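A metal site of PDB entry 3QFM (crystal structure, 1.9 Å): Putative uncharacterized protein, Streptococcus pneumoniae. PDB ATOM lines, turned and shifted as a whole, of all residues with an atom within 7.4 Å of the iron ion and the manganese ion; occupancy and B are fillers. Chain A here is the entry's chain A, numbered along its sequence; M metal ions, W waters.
A ring nitrogen (ND1) of His 21 is in hydrogen-bond range of the backbone carbonyl oxygen (O) of Met 50, at 2.8 Å. The backbone NH (N) of Ile 20 lies within hydrogen-bond range of the backbone carbonyl oxygen (O) of Asp 47 (3.1 Å). The side-chain hydroxyl (OG) of Ser 192 is in hydrogen-bond range of the backbone carbonyl oxygen (O) of Asp 19 (2.6 Å). The backbone carbonyl oxygen (O) of His 136 is in hydrogen-bond range of the backbone NH (N) of Gly 171 (2.9 Å). The side-chain carboxylate (OD1) of Asp 47 sits at hydrogen-bond distance from the backbone NH (N) of Trp 75. The side-chain carboxylate (OD1) of Asp 19 lies within hydrogen-bond range of the side-chain hydroxyl (OG) of Ser 18 (2.7 Å). A ring nitrogen (NE2) of His 172 sits at hydrogen-bond distance from the backbone carbonyl oxygen (O) of Gly 144, 2.8 Å away. ND1 of His 174 is in hydrogen-bond range of O of Gln 195 (2.8 Å).
Of the 26 residues printed, 5 come within 4 Å of the manganese ion. The nearest printed residue that does not touch the manganese ion is Asn 142 (4.2 Å).
The iron ion is bound by water W1 (1.9 Å), OD2 of Asp 19 (2.1 Å), NE2 of His 21 (2.2 Å), OD2 of Asp 47 (2.3 Å) and NE2 of His 174 (2.3 Å). The iron ion has five donor atoms within binding distance.
The manganese ion is bound by water W1 (2.0 Å), OD1 of Asn 74 (2.1 Å), NE2 of His 136 (2.2 Å), OD2 of Asp 47 (2.3 Å) and ND1 of His 172 (2.3 Å).
Water W2 lies within hydrogen-bond range of the backbone carbonyl oxygen of Phe 267, the indole nitrogen of Trp 75 and the side-chain amide nitrogen of Asn 74.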
ATOM      1  N   SER A  18       1.925 -20.664   1.172  1.00  0.00           N
ATOM      2  CA  SER A  18       1.068 -20.134   2.235  1.00  0.00           C
ATOM      3  C   SER A  18      -0.214 -19.471   1.687  1.00  0.00           C
ATOM      4  O   SER A  18      -0.186 -18.861   0.598  1.00  0.00           O
ATOM      5  CB  SER A  18       1.845 -19.074   3.037  1.00  0.00           C
ATOM      6  OG  SER A  18       1.196 -18.863   4.294  1.00  0.00           O
ATOM      7  N   ASP A  19      -1.300 -19.563   2.444  1.00  0.00           N
ATOM      8  CA  ASP A  19      -2.486 -18.738   2.180  1.00  0.00           C
ATOM      9  C   ASP A  19      -2.950 -18.916   0.729  1.00  0.00           C
ATOM     10  O   ASP A  19      -3.113 -17.948  -0.061  1.00  0.00           O
ATOM     11  CB  ASP A  19      -2.153 -17.257   2.520  1.00  0.00           C
ATOM     12  CG  ASP A  19      -1.810 -17.081   3.998  1.00  0.00           C
ATOM     13  OD1 ASP A  19      -0.633 -16.945   4.344  1.00  0.00           O
ATOM     14  OD2 ASP A  19      -2.720 -17.139   4.843  1.00  0.00           O
ATOM     15  N   ILE A  20      -3.124 -20.182   0.369  1.00  0.00           N
ATOM     16  CA  ILE A  20      -3.674 -20.575  -0.927  1.00  0.00           C
ATOM     17  C   ILE A  20      -5.138 -20.140  -1.047  1.00  0.00           C
ATOM     18  O   ILE A  20      -5.580 -19.677  -2.110  1.00  0.00           O
ATOM     19  CB  ILE A  20      -3.541 -22.131  -1.107  1.00  0.00           C
ATOM     20  CG1 ILE A  20      -2.071 -22.519  -1.013  1.00  0.00           C
ATOM     21  CG2 ILE A  20      -4.168 -22.623  -2.408  1.00  0.00           C
ATOM     22  CD1 ILE A  20      -1.846 -24.032  -0.734  1.00  0.00           C
ATOM     23  N   HIS A  21      -5.877 -20.294   0.036  1.00  0.00           N
ATOM     24  CA  HIS A  21      -7.243 -19.795   0.139  1.00  0.00           C
ATOM     25  C   HIS A  21      -8.137 -20.290  -1.016  1.00  0.00           C
ATOM     26  O   HIS A  21      -8.990 -19.564  -1.555  1.00  0.00           O
ATOM     27  CB  HIS A  21      -7.238 -18.270   0.274  1.00  0.00           C
ATOM     28  CG  HIS A  21      -6.957 -17.808   1.665  1.00  0.00           C
ATOM     29  ND1 HIS A  21      -7.835 -18.004   2.708  1.00  0.00           N
ATOM     30  CD2 HIS A  21      -5.845 -17.230   2.213  1.00  0.00           C
ATOM     31  CE1 HIS A  21      -7.306 -17.547   3.828  1.00  0.00           C
ATOM     32  NE2 HIS A  21      -6.106 -17.065   3.545  1.00  0.00           N
ATOM     33  N   LEU A  45       2.173 -23.604   5.065  1.00  0.00           N
ATOM     34  CA  LEU A  45       1.986 -22.702   6.199  1.00  0.00           C
ATOM     35  C   LEU A  45       0.531 -22.497   6.601  1.00  0.00           C
ATOM     36  O   LEU A  45       0.262 -21.733   7.526  1.00  0.00           O
ATOM     37  CB  LEU A  45       2.661 -21.323   5.954  1.00  0.00           C
ATOM     38  CG  LEU A  45       4.154 -21.290   5.588  1.00  0.00           C
ATOM     39  CD1 LEU A  45       4.768 -19.922   5.933  1.00  0.00           C
ATOM     40  CD2 LEU A  45       4.993 -22.418   6.230  1.00  0.00           C
ATOM     41  N   GLY A  46      -0.401 -23.203   5.939  1.00  0.00           N
ATOM     42  CA  GLY A  46      -1.812 -23.100   6.296  1.00  0.00           C
ATOM     43  C   GLY A  46      -2.691 -22.126   5.494  1.00  0.00           C
ATOM     44  O   GLY A  46      -2.206 -21.388   4.601  1.00  0.00           O
ATOM     45  N   ASP A  47      -3.983 -22.140   5.817  1.00  0.00           N
ATOM     46  CA  ASP A  47      -5.019 -21.380   5.073  1.00  0.00           C
ATOM     47  C   ASP A  47      -5.141 -21.927   3.657  1.00  0.00           C
ATOM     48  O   ASP A  47      -4.856 -21.254   2.643  1.00  0.00           O
ATOM     49  CB  ASP A  47      -4.769 -19.860   5.119  1.00  0.00           C
ATOM     50  CG  ASP A  47      -5.192 -19.244   6.417  1.00  0.00           C
ATOM     51  OD1 ASP A  47      -5.549 -20.017   7.343  1.00  0.00           O
ATOM     52  OD2 ASP A  47      -5.157 -17.994   6.521  1.00  0.00           O
ATOM     53  N   ILE A  48      -5.544 -23.200   3.603  1.00  0.00           N
ATOM     54  CA  ILE A  48      -5.525 -23.963   2.374  1.00  0.00           C
ATOM     55  C   ILE A  48      -6.774 -23.760   1.503  1.00  0.00           C
ATOM     56  O   ILE A  48      -6.671 -23.444   0.314  1.00  0.00           O
ATOM     57  CB  ILE A  48      -5.328 -25.463   2.709  1.00  0.00           C
ATOM     58  CG1 ILE A  48      -4.006 -25.632   3.489  1.00  0.00           C
ATOM     59  CG2 ILE A  48      -5.351 -26.313   1.439  1.00  0.00           C
ATOM     60  CD1 ILE A  48      -3.932 -27.027   4.182  1.00  0.00           C
ATOM     61  N   MET A  50     -10.809 -22.051   0.945  1.00  0.00           N
ATOM     62  CA  MET A  50     -11.755 -20.937   1.153  1.00  0.00           C
ATOM     63  C   MET A  50     -11.022 -19.600   1.173  1.00  0.00           C
ATOM     64  O   MET A  50      -9.934 -19.522   1.719  1.00  0.00           O
ATOM     65  CB  MET A  50     -12.564 -21.093   2.444  1.00  0.00           C
ATOM     66  CG  MET A  50     -13.288 -22.438   2.564  1.00  0.00           C
ATOM     67  SD  MET A  50     -14.263 -22.510   4.069  1.00  0.00           S
ATOM     68  CE  MET A  50     -13.046 -22.261   5.349  1.00  0.00           C
ATOM     69  N   LEU A  72      -0.905 -25.463  11.123  1.00  0.00           N
ATOM     70  CA  LEU A  72      -2.321 -25.108  11.146  1.00  0.00           C
ATOM     71  C   LEU A  72      -2.625 -23.608  10.958  1.00  0.00           C
ATOM     72  O   LEU A  72      -2.209 -22.788  11.773  1.00  0.00           O
ATOM     73  CB  LEU A  72      -2.924 -25.539  12.477  1.00  0.00           C
ATOM     74  CG  LEU A  72      -4.437 -25.438  12.679  1.00  0.00           C
ATOM     75  CD1 LEU A  72      -5.198 -26.504  11.825  1.00  0.00           C
ATOM     76  CD2 LEU A  72      -4.717 -25.652  14.152  1.00  0.00           C
ATOM     77  N   GLY A  73      -3.437 -23.311   9.947  1.00  0.00           N
ATOM     78  CA  GLY A  73      -3.911 -21.944   9.709  1.00  0.00           C
ATOM     79  C   GLY A  73      -5.243 -21.690  10.384  1.00  0.00           C
ATOM     80  O   GLY A  73      -6.017 -22.632  10.637  1.00  0.00           O
ATOM     81  N   ASN A  74      -5.539 -20.431  10.654  1.00  0.00           N
ATOM     82  CA  ASN A  74      -6.861 -20.118  11.223  1.00  0.00           C
ATOM     83  C   ASN A  74      -8.077 -20.556  10.381  1.00  0.00           C
ATOM     84  O   ASN A  74      -9.107 -20.949  10.951  1.00  0.00           O
ATOM     85  CB  ASN A  74      -6.960 -18.643  11.646  1.00  0.00           C
ATOM     86  CG  ASN A  74      -6.756 -17.662  10.499  1.00  0.00           C
ATOM     87  OD1 ASN A  74      -5.783 -17.776   9.696  1.00  0.00           O
ATOM     88  ND2 ASN A  74      -7.658 -16.657  10.429  1.00  0.00           N
ATOM     89  N   TRP A  75      -7.957 -20.521   9.066  1.00  0.00           N
ATOM     90  CA  TRP A  75      -9.064 -20.970   8.187  1.00  0.00           C
ATOM     91  C   TRP A  75      -9.324 -22.490   8.232  1.00  0.00           C
ATOM     92  O   TRP A  75     -10.413 -22.945   7.863  1.00  0.00           O
ATOM     93  CB  TRP A  75      -8.867 -20.480   6.746  1.00  0.00           C
ATOM     94  CG  TRP A  75      -9.140 -18.998   6.624  1.00  0.00           C
ATOM     95  CD1 TRP A  75      -8.444 -17.970   7.221  1.00  0.00           C
ATOM     96  CD2 TRP A  75     -10.179 -18.378   5.858  1.00  0.00           C
ATOM     97  NE1 TRP A  75      -8.997 -16.756   6.870  1.00  0.00           N
ATOM     98  CE2 TRP A  75     -10.060 -16.975   6.029  1.00  0.00           C
ATOM     99  CE3 TRP A  75     -11.198 -18.872   5.032  1.00  0.00           C
ATOM    100  CZ2 TRP A  75     -10.929 -16.057   5.409  1.00  0.00           C
ATOM    101  CZ3 TRP A  75     -12.074 -17.960   4.406  1.00  0.00           C
ATOM    102  CH2 TRP A  75     -11.925 -16.563   4.609  1.00  0.00           C
ATOM    103  N   HIS A 136       1.800 -20.541  11.352  1.00  0.00           N
ATOM    104  CA  HIS A 136       0.974 -19.745  10.451  1.00  0.00           C
ATOM    105  C   HIS A 136       1.036 -18.262  10.851  1.00  0.00           C
ATOM    106  O   HIS A 136       1.270 -17.397  10.037  1.00  0.00           O
ATOM    107  CB  HIS A 136      -0.497 -20.188  10.507  1.00  0.00           C
ATOM    108  CG  HIS A 136      -1.366 -19.434   9.547  1.00  0.00           C
ATOM    109  ND1 HIS A 136      -1.209 -19.534   8.177  1.00  0.00           N
ATOM    110  CD2 HIS A 136      -2.390 -18.576   9.751  1.00  0.00           C
ATOM    111  CE1 HIS A 136      -2.115 -18.791   7.580  1.00  0.00           C
ATOM    112  NE2 HIS A 136      -2.836 -18.184   8.503  1.00  0.00           N
ATOM    113  N   HIS A 137       0.821 -17.995  12.120  1.00  0.00           N
ATOM    114  CA  HIS A 137       0.960 -16.642  12.614  1.00  0.00           C
ATOM    115  C   HIS A 137       1.923 -16.719  13.808  1.00  0.00           C
ATOM    116  O   HIS A 137       3.104 -17.038  13.617  1.00  0.00           O
ATOM    117  CB  HIS A 137      -0.446 -16.108  12.962  1.00  0.00           C
ATOM    118  CG  HIS A 137      -0.460 -14.667  13.366  1.00  0.00           C
ATOM    119  ND1 HIS A 137      -1.308 -14.188  14.342  1.00  0.00           N
ATOM    120  CD2 HIS A 137       0.294 -13.615  12.957  1.00  0.00           C
ATOM    121  CE1 HIS A 137      -1.116 -12.888  14.475  1.00  0.00           C
ATOM    122  NE2 HIS A 137      -0.143 -12.513  13.656  1.00  0.00           N
ATOM    123  N   ASN A 142      -2.958 -18.779  15.805  1.00  0.00           N
ATOM    124  CA  ASN A 142      -2.924 -18.702  14.316  1.00  0.00           C
ATOM    125  C   ASN A 142      -3.780 -17.602  13.670  1.00  0.00           C
ATOM    126  O   ASN A 142      -3.937 -17.574  12.434  1.00  0.00           O
ATOM    127  CB  ASN A 142      -3.187 -20.064  13.663  1.00  0.00           C
ATOM    128  CG  ASN A 142      -4.585 -20.625  13.921  1.00  0.00           C
ATOM    129  OD1 ASN A 142      -5.484 -19.907  14.373  1.00  0.00           O
ATOM    130  ND2 ASN A 142      -4.775 -21.902  13.634  1.00  0.00           N
ATOM    131  N   TRP A 143      -4.316 -16.719  14.503  1.00  0.00           N
ATOM    132  CA  TRP A 143      -5.238 -15.662  14.049  1.00  0.00           C
ATOM    133  C   TRP A 143      -4.882 -14.340  14.723  1.00  0.00           C
ATOM    134  O   TRP A 143      -4.120 -14.327  15.684  1.00  0.00           O
ATOM    135  CB  TRP A 143      -6.701 -16.043  14.399  1.00  0.00           C
ATOM    136  CG  TRP A 143      -6.900 -16.324  15.880  1.00  0.00           C
ATOM    137  CD1 TRP A 143      -6.628 -17.508  16.531  1.00  0.00           C
ATOM    138  CD2 TRP A 143      -7.373 -15.425  16.880  1.00  0.00           C
ATOM    139  NE1 TRP A 143      -6.907 -17.399  17.855  1.00  0.00           N
ATOM    140  CE2 TRP A 143      -7.376 -16.135  18.105  1.00  0.00           C
ATOM    141  CE3 TRP A 143      -7.814 -14.092  16.867  1.00  0.00           C
ATOM    142  CZ2 TRP A 143      -7.814 -15.553  19.303  1.00  0.00           C
ATOM    143  CZ3 TRP A 143      -8.234 -13.511  18.064  1.00  0.00           C
ATOM    144  CH2 TRP A 143      -8.221 -14.245  19.261  1.00  0.00           C
ATOM    145  N   GLY A 144      -5.435 -13.251  14.209  1.00  0.00           N
ATOM    146  CA  GLY A 144      -5.209 -11.928  14.795  1.00  0.00           C
ATOM    147  C   GLY A 144      -4.345 -10.999  13.969  1.00  0.00           C
ATOM    148  O   GLY A 144      -3.983 -11.308  12.819  1.00  0.00           O
ATOM    149  N   GLY A 171       3.123 -16.958   7.816  1.00  0.00           N
ATOM    150  CA  GLY A 171       2.264 -16.515   6.697  1.00  0.00           C
ATOM    151  C   GLY A 171       1.174 -15.606   7.278  1.00  0.00           C
ATOM    152  O   GLY A 171       1.503 -14.660   7.978  1.00  0.00           O
ATOM    153  N   HIS A 172      -0.101 -15.903   7.012  1.00  0.00           N
ATOM    154  CA  HIS A 172      -1.255 -15.203   7.653  1.00  0.00           C
ATOM    155  C   HIS A 172      -1.537 -13.753   7.180  1.00  0.00           C
ATOM    156  O   HIS A 172      -2.687 -13.370   6.950  1.00  0.00           O
ATOM    157  CB  HIS A 172      -1.172 -15.235   9.204  1.00  0.00           C
ATOM    158  CG  HIS A 172      -2.385 -14.668   9.884  1.00  0.00           C
ATOM    159  ND1 HIS A 172      -3.649 -15.209   9.713  1.00  0.00           N
ATOM    160  CD2 HIS A 172      -2.537 -13.614  10.722  1.00  0.00           C
ATOM    161  CE1 HIS A 172      -4.524 -14.504  10.435  1.00  0.00           C
ATOM    162  NE2 HIS A 172      -3.868 -13.546  11.068  1.00  0.00           N
ATOM    163  N   ILE A 173      -0.496 -12.936   7.068  1.00  0.00           N
ATOM    164  CA  ILE A 173      -0.713 -11.525   6.706  1.00  0.00           C
ATOM    165  C   ILE A 173      -0.762 -11.216   5.206  1.00  0.00           C
ATOM    166  O   ILE A 173      -1.156 -10.109   4.839  1.00  0.00           O
ATOM    167  CB  ILE A 173       0.270 -10.590   7.461  1.00  0.00           C
ATOM    168  CG1 ILE A 173       1.717 -10.822   7.001  1.00  0.00           C
ATOM    169  CG2 ILE A 173       0.112 -10.819   8.966  1.00  0.00           C
ATOM    170  CD1 ILE A 173       2.664  -9.632   7.353  1.00  0.00           C
ATOM    171  N   HIS A 174      -0.419 -12.208   4.360  1.00  0.00           N
ATOM    172  CA  HIS A 174      -0.498 -12.090   2.897  1.00  0.00           C
ATOM    173  C   HIS A 174       0.431 -10.993   2.322  1.00  0.00           C
ATOM    174  O   HIS A 174       0.109 -10.360   1.303  1.00  0.00           O
ATOM    175  CB  HIS A 174      -1.933 -11.829   2.419  1.00  0.00           C
ATOM    176  CG  HIS A 174      -2.918 -12.885   2.828  1.00  0.00           C
ATOM    177  ND1 HIS A 174      -4.125 -13.019   2.193  1.00  0.00           N
ATOM    178  CD2 HIS A 174      -2.879 -13.847   3.778  1.00  0.00           C
ATOM    179  CE1 HIS A 174      -4.789 -14.035   2.730  1.00  0.00           C
ATOM    180  NE2 HIS A 174      -4.056 -14.547   3.705  1.00  0.00           N
ATOM    181  N   SER A 192       1.103 -14.512   0.098  1.00  0.00           N
ATOM    182  CA  SER A 192      -0.074 -15.370  -0.157  1.00  0.00           C
ATOM    183  C   SER A 192      -0.132 -15.814  -1.600  1.00  0.00           C
ATOM    184  O   SER A 192      -0.034 -15.001  -2.526  1.00  0.00           O
ATOM    185  CB  SER A 192      -1.380 -14.608   0.183  1.00  0.00           C
ATOM    186  OG  SER A 192      -2.512 -15.374  -0.162  1.00  0.00           O
ATOM    187  N   GLN A 195      -4.435 -14.903  -2.332  1.00  0.00           N
ATOM    188  CA  GLN A 195      -5.056 -13.635  -1.905  1.00  0.00           C
ATOM    189  C   GLN A 195      -3.983 -12.593  -1.537  1.00  0.00           C
ATOM    190  O   GLN A 195      -3.974 -12.084  -0.422  1.00  0.00           O
ATOM    191  CB  GLN A 195      -5.988 -13.849  -0.694  1.00  0.00           C
ATOM    192  CG  GLN A 195      -7.120 -14.863  -0.866  1.00  0.00           C
ATOM    193  CD  GLN A 195      -8.332 -14.300  -1.613  1.00  0.00           C
ATOM    194  OE1 GLN A 195      -9.353 -13.983  -1.009  1.00  0.00           O
ATOM    195  NE2 GLN A 195      -8.206 -14.172  -2.934  1.00  0.00           N
ATOM    196  N   PHE A 267     -10.012 -11.365   7.092  1.00  0.00           N
ATOM    197  CA  PHE A 267      -8.746 -12.104   7.253  1.00  0.00           C
ATOM    198  C   PHE A 267      -8.052 -11.783   8.588  1.00  0.00           C
ATOM    199  O   PHE A 267      -7.464 -12.670   9.228  1.00  0.00           O
ATOM    200  CB  PHE A 267      -7.788 -11.799   6.097  1.00  0.00           C
ATOM    201  CG  PHE A 267      -8.174 -12.410   4.760  1.00  0.00           C
ATOM    202  CD1 PHE A 267      -8.387 -11.599   3.645  1.00  0.00           C
ATOM    203  CD2 PHE A 267      -8.281 -13.795   4.611  1.00  0.00           C
ATOM    204  CE1 PHE A 267      -8.724 -12.149   2.411  1.00  0.00           C
ATOM    205  CE2 PHE A 267      -8.624 -14.360   3.384  1.00  0.00           C
ATOM    206  CZ  PHE A 267      -8.842 -13.542   2.266  1.00  0.00           C
ATOM    207  N   LEU A 268      -8.108 -10.514   8.999  1.00  0.00           N
ATOM    208  CA  LEU A 268      -7.324 -10.011  10.117  1.00  0.00           C
ATOM    209  C   LEU A 268      -8.209  -9.407  11.220  1.00  0.00           C
ATOM    210  O   LEU A 268      -8.563 -10.095  12.196  1.00  0.00           O
ATOM    211  CB  LEU A 268      -6.301  -8.967   9.597  1.00  0.00           C
ATOM    212  CG  LEU A 268      -5.281  -9.429   8.533  1.00  0.00           C
ATOM    213  CD1 LEU A 268      -4.637  -8.244   7.788  1.00  0.00           C
ATOM    214  CD2 LEU A 268      -4.211 -10.362   9.094  1.00  0.00           C
HETATM  215 FE    FE M   1      -4.676 -16.354   5.011  1.00  0.00          FE
HETATM  216 MN    MN M   2      -4.510 -16.793   8.327  1.00  0.00          MN
HETATM  217  O   HOH W   1      -4.568 -15.580   6.718  1.00  0.00           O
HETATM  218  O   HOH W   2      -7.033 -14.974   7.927  1.00  0.00           O
